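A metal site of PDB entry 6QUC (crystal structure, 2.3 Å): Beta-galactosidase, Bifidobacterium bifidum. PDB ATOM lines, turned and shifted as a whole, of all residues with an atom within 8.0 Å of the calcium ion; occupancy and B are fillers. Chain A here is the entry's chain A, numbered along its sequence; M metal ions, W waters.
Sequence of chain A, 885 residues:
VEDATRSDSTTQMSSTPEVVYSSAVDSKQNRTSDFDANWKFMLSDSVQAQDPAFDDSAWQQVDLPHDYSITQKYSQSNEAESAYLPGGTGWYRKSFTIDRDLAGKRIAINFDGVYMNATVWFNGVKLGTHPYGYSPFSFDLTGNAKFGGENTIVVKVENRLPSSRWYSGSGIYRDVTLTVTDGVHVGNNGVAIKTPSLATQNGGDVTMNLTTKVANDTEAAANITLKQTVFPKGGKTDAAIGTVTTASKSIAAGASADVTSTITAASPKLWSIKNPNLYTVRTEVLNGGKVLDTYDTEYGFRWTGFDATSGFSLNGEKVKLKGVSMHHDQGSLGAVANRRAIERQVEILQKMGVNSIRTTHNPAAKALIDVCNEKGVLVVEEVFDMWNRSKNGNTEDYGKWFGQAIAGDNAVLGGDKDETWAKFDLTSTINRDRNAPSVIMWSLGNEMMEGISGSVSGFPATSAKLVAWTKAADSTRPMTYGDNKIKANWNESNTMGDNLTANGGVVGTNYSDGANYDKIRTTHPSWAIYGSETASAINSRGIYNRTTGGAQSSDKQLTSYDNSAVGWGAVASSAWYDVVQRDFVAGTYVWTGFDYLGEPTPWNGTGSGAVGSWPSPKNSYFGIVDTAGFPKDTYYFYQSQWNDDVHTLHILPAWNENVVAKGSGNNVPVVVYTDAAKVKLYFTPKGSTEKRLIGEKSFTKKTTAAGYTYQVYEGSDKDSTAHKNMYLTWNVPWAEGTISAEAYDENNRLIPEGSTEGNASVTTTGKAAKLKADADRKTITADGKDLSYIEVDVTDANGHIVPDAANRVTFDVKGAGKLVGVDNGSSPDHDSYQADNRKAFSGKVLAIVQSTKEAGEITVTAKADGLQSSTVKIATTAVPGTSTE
The calcium ion is bound by OD1 of Asn 394 (2.3 Å), OE2 of Glu 81 (2.4 Å), O of Thr 606 (2.4 Å), water W1 (2.4 Å), OE1 of Glu 79 (2.4 Å) and O of Asn 392 (2.5 Å). The calcium ion has six donor atoms within binding distance.
Water W1 lies within hydrogen-bond range of O of Gly 393 (2.8 Å) and OE2 of Glu 79 (2.8 Å).
ND2 of Asn 394 lies close to O of Lys 391 (3.2 Å). ND2 of Asn 394 sits close to O of Ser 164 (3.4 Å). N of Glu 81 sits at hydrogen-bond distance from O of Gly 605 (3.2 Å). O of Glu 79 sits at hydrogen-bond distance from OG of Ser 82.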
ATOM      1  N   GLU A  79      -5.070  -8.258  25.792  1.00  0.00           N
ATOM      2  CA  GLU A  79      -6.257  -8.452  26.613  1.00  0.00           C
ATOM      3  C   GLU A  79      -6.119  -9.714  27.465  1.00  0.00           C
ATOM      4  O   GLU A  79      -5.636 -10.745  26.992  1.00  0.00           O
ATOM      5  CB  GLU A  79      -7.525  -8.533  25.750  1.00  0.00           C
ATOM      6  CG  GLU A  79      -7.705  -7.332  24.852  1.00  0.00           C
ATOM      7  CD  GLU A  79      -9.141  -7.124  24.405  1.00  0.00           C
ATOM      8  OE1 GLU A  79      -9.977  -8.039  24.586  1.00  0.00           O
ATOM      9  OE2 GLU A  79      -9.440  -6.032  23.875  1.00  0.00           O
ATOM     10  N   ALA A  80      -6.572  -9.621  28.725  1.00  0.00           N
ATOM     11  CA  ALA A  80      -6.427 -10.734  29.645  1.00  0.00           C
ATOM     12  C   ALA A  80      -7.226 -11.946  29.203  1.00  0.00           C
ATOM     13  O   ALA A  80      -6.770 -13.096  29.351  1.00  0.00           O
ATOM     14  CB  ALA A  80      -6.850 -10.310  31.052  1.00  0.00           C
ATOM     15  N   GLU A  81      -8.422 -11.738  28.654  1.00  0.00           N
ATOM     16  CA  GLU A  81      -9.291 -12.867  28.330  1.00  0.00           C
ATOM     17  C   GLU A  81      -8.683 -13.739  27.229  1.00  0.00           C
ATOM     18  O   GLU A  81      -8.969 -14.945  27.170  1.00  0.00           O
ATOM     19  CB  GLU A  81     -10.676 -12.377  27.939  1.00  0.00           C
ATOM     20  CG  GLU A  81     -10.731 -11.499  26.698  1.00  0.00           C
ATOM     21  CD  GLU A  81     -12.155 -11.061  26.369  1.00  0.00           C
ATOM     22  OE1 GLU A  81     -13.109 -11.646  26.933  1.00  0.00           O
ATOM     23  OE2 GLU A  81     -12.323 -10.132  25.554  1.00  0.00           O
ATOM     24  N   SER A  82      -7.836 -13.173  26.368  1.00  0.00           N
ATOM     25  CA  SER A  82      -7.104 -13.933  25.375  1.00  0.00           C
ATOM     26  C   SER A  82      -5.637 -14.120  25.767  1.00  0.00           C
ATOM     27  O   SER A  82      -4.768 -14.212  24.882  1.00  0.00           O
ATOM     28  CB  SER A  82      -7.220 -13.279  23.997  1.00  0.00           C
ATOM     29  OG  SER A  82      -6.841 -11.911  24.052  1.00  0.00           O
ATOM     30  N   LEU A 161      -6.530  -8.951  16.714  1.00  0.00           N
ATOM     31  CA  LEU A 161      -7.168  -8.820  18.006  1.00  0.00           C
ATOM     32  C   LEU A 161      -8.029  -7.568  18.035  1.00  0.00           C
ATOM     33  O   LEU A 161      -7.750  -6.600  17.317  1.00  0.00           O
ATOM     34  CB  LEU A 161      -6.150  -8.766  19.140  1.00  0.00           C
ATOM     35  CG  LEU A 161      -5.432 -10.034  19.614  1.00  0.00           C
ATOM     36  CD1 LEU A 161      -4.886 -10.890  18.494  1.00  0.00           C
ATOM     37  CD2 LEU A 161      -4.319  -9.647  20.593  1.00  0.00           C
ATOM     38  N   PRO A 162      -9.094  -7.543  18.850  1.00  0.00           N
ATOM     39  CA  PRO A 162      -9.583  -8.645  19.695  1.00  0.00           C
ATOM     40  C   PRO A 162     -10.706  -9.442  19.034  1.00  0.00           C
ATOM     41  O   PRO A 162     -11.649  -8.864  18.490  1.00  0.00           O
ATOM     42  CB  PRO A 162     -10.080  -7.930  20.940  1.00  0.00           C
ATOM     43  CG  PRO A 162     -10.578  -6.611  20.425  1.00  0.00           C
ATOM     44  CD  PRO A 162      -9.778  -6.275  19.176  1.00  0.00           C
ATOM     45  N   SER A 163     -10.618 -10.781  19.096  1.00  0.00           N
ATOM     46  CA  SER A 163     -11.574 -11.639  18.410  1.00  0.00           C
ATOM     47  C   SER A 163     -12.105 -12.783  19.265  1.00  0.00           C
ATOM     48  O   SER A 163     -12.822 -13.640  18.742  1.00  0.00           O
ATOM     49  CB  SER A 163     -10.942 -12.231  17.144  1.00  0.00           C
ATOM     50  OG  SER A 163      -9.987 -13.217  17.488  1.00  0.00           O
ATOM     51  N   SER A 164     -11.793 -12.828  20.565  1.00  0.00           N
ATOM     52  CA  SER A 164     -12.098 -14.044  21.311  1.00  0.00           C
ATOM     53  C   SER A 164     -12.179 -13.756  22.796  1.00  0.00           C
ATOM     54  O   SER A 164     -11.420 -12.950  23.341  1.00  0.00           O
ATOM     55  CB  SER A 164     -11.028 -15.108  21.043  1.00  0.00           C
ATOM     56  OG  SER A 164     -11.358 -16.346  21.667  1.00  0.00           O
ATOM     57  N   ARG A 165     -13.118 -14.433  23.468  1.00  0.00           N
ATOM     58  CA  ARG A 165     -13.250 -14.420  24.918  1.00  0.00           C
ATOM     59  C   ARG A 165     -12.290 -15.383  25.608  1.00  0.00           C
ATOM     60  O   ARG A 165     -12.283 -15.450  26.837  1.00  0.00           O
ATOM     61  CB  ARG A 165     -14.699 -14.737  25.324  1.00  0.00           C
ATOM     62  CG  ARG A 165     -15.729 -13.790  24.732  1.00  0.00           C
ATOM     63  CD  ARG A 165     -17.123 -13.988  25.341  1.00  0.00           C
ATOM     64  NE  ARG A 165     -17.685 -15.301  25.029  1.00  0.00           N
ATOM     65  CZ  ARG A 165     -17.686 -16.328  25.868  1.00  0.00           C
ATOM     66  NH1 ARG A 165     -17.161 -16.215  27.080  1.00  0.00           N
ATOM     67  NH2 ARG A 165     -18.220 -17.488  25.493  1.00  0.00           N
ATOM     68  N   LYS A 391     -19.236  -9.982  21.202  1.00  0.00           N
ATOM     69  CA  LYS A 391     -19.184 -10.034  22.654  1.00  0.00           C
ATOM     70  C   LYS A 391     -17.942  -9.327  23.174  1.00  0.00           C
ATOM     71  O   LYS A 391     -16.895  -9.331  22.528  1.00  0.00           O
ATOM     72  CB  LYS A 391     -19.175 -11.485  23.164  1.00  0.00           C
ATOM     73  CG  LYS A 391     -20.417 -12.289  22.859  1.00  0.00           C
ATOM     74  CD  LYS A 391     -20.371 -13.619  23.574  1.00  0.00           C
ATOM     75  CE  LYS A 391     -21.644 -14.426  23.379  1.00  0.00           C
ATOM     76  NZ  LYS A 391     -21.548 -15.746  24.045  1.00  0.00           N
ATOM     77  N   ASN A 392     -18.069  -8.735  24.364  1.00  0.00           N
ATOM     78  CA  ASN A 392     -16.927  -8.310  25.176  1.00  0.00           C
ATOM     79  C   ASN A 392     -16.012  -7.352  24.421  1.00  0.00           C
ATOM     80  O   ASN A 392     -14.786  -7.400  24.552  1.00  0.00           O
ATOM     81  CB  ASN A 392     -16.145  -9.524  25.685  1.00  0.00           C
ATOM     82  CG  ASN A 392     -16.974 -10.432  26.589  1.00  0.00           C
ATOM     83  OD1 ASN A 392     -18.205 -10.357  26.601  1.00  0.00           O
ATOM     84  ND2 ASN A 392     -16.294 -11.285  27.341  1.00  0.00           N
ATOM     85  N   GLY A 393     -16.609  -6.482  23.604  1.00  0.00           N
ATOM     86  CA  GLY A 393     -15.826  -5.539  22.814  1.00  0.00           C
ATOM     87  C   GLY A 393     -14.919  -6.170  21.790  1.00  0.00           C
ATOM     88  O   GLY A 393     -13.998  -5.508  21.300  1.00  0.00           O
ATOM     89  N   ASN A 394     -15.144  -7.434  21.434  1.00  0.00           N
ATOM     90  CA  ASN A 394     -14.295  -8.131  20.471  1.00  0.00           C
ATOM     91  C   ASN A 394     -14.807  -7.819  19.070  1.00  0.00           C
ATOM     92  O   ASN A 394     -15.570  -8.579  18.458  1.00  0.00           O
ATOM     93  CB  ASN A 394     -14.287  -9.632  20.756  1.00  0.00           C
ATOM     94  CG  ASN A 394     -13.665  -9.961  22.093  1.00  0.00           C
ATOM     95  OD1 ASN A 394     -12.756  -9.266  22.546  1.00  0.00           O
ATOM     96  ND2 ASN A 394     -14.164 -11.003  22.746  1.00  0.00           N
ATOM     97  N   THR A 395     -14.362  -6.673  18.556  1.00  0.00           N
ATOM     98  CA  THR A 395     -14.819  -6.167  17.269  1.00  0.00           C
ATOM     99  C   THR A 395     -14.385  -7.033  16.094  1.00  0.00           C
ATOM    100  O   THR A 395     -14.908  -6.860  14.991  1.00  0.00           O
ATOM    101  CB  THR A 395     -14.311  -4.731  17.050  1.00  0.00           C
ATOM    102  OG1 THR A 395     -12.874  -4.703  17.116  1.00  0.00           O
ATOM    103  CG2 THR A 395     -14.883  -3.787  18.100  1.00  0.00           C
ATOM    104  N   ASP A 397     -14.393 -10.533  16.317  1.00  0.00           N
ATOM    105  CA  ASP A 397     -14.901 -11.894  16.450  1.00  0.00           C
ATOM    106  C   ASP A 397     -15.864 -12.218  15.310  1.00  0.00           C
ATOM    107  O   ASP A 397     -16.101 -11.412  14.400  1.00  0.00           O
ATOM    108  CB  ASP A 397     -15.522 -12.099  17.837  1.00  0.00           C
ATOM    109  CG  ASP A 397     -16.814 -11.315  18.048  1.00  0.00           C
ATOM    110  OD1 ASP A 397     -17.388 -10.765  17.079  1.00  0.00           O
ATOM    111  OD2 ASP A 397     -17.262 -11.243  19.216  1.00  0.00           O
ATOM    112  N   GLY A 605     -10.148  -9.653  32.054  1.00  0.00           N
ATOM    113  CA  GLY A 605     -10.227  -8.329  31.479  1.00  0.00           C
ATOM    114  C   GLY A 605     -10.729  -8.363  30.050  1.00  0.00           C
ATOM    115  O   GLY A 605     -10.170  -9.067  29.208  1.00  0.00           O
ATOM    116  N   THR A 606     -11.791  -7.615  29.765  1.00  0.00           N
ATOM    117  CA  THR A 606     -12.335  -7.593  28.408  1.00  0.00           C
ATOM    118  C   THR A 606     -11.701  -6.523  27.530  1.00  0.00           C
ATOM    119  O   THR A 606     -11.809  -6.614  26.300  1.00  0.00           O
ATOM    120  CB  THR A 606     -13.846  -7.372  28.437  1.00  0.00           C
ATOM    121  OG1 THR A 606     -14.136  -6.192  29.209  1.00  0.00           O
ATOM    122  CG2 THR A 606     -14.562  -8.577  29.041  1.00  0.00           C
ATOM    123  N   GLY A 607     -11.026  -5.532  28.119  1.00  0.00           N
ATOM    124  CA  GLY A 607     -10.245  -4.583  27.379  1.00  0.00           C
ATOM    125  C   GLY A 607      -8.753  -4.833  27.527  1.00  0.00           C
ATOM    126  O   GLY A 607      -8.310  -5.828  28.091  1.00  0.00           O
ATOM    127  N   SER A 608      -7.975  -3.884  27.008  1.00  0.00           N
ATOM    128  CA  SER A 608      -6.529  -3.985  27.140  1.00  0.00           C
ATOM    129  C   SER A 608      -6.091  -3.509  28.517  1.00  0.00           C
ATOM    130  O   SER A 608      -6.801  -2.788  29.219  1.00  0.00           O
ATOM    131  CB  SER A 608      -5.830  -3.188  26.041  1.00  0.00           C
ATOM    132  OG  SER A 608      -6.070  -1.806  26.180  1.00  0.00           O
HETATM  133 CA    CA M   1     -12.384  -8.026  24.497  1.00  0.00          CA
HETATM  134  O   HOH W   1     -12.177  -5.962  23.317  1.00  0.00           O
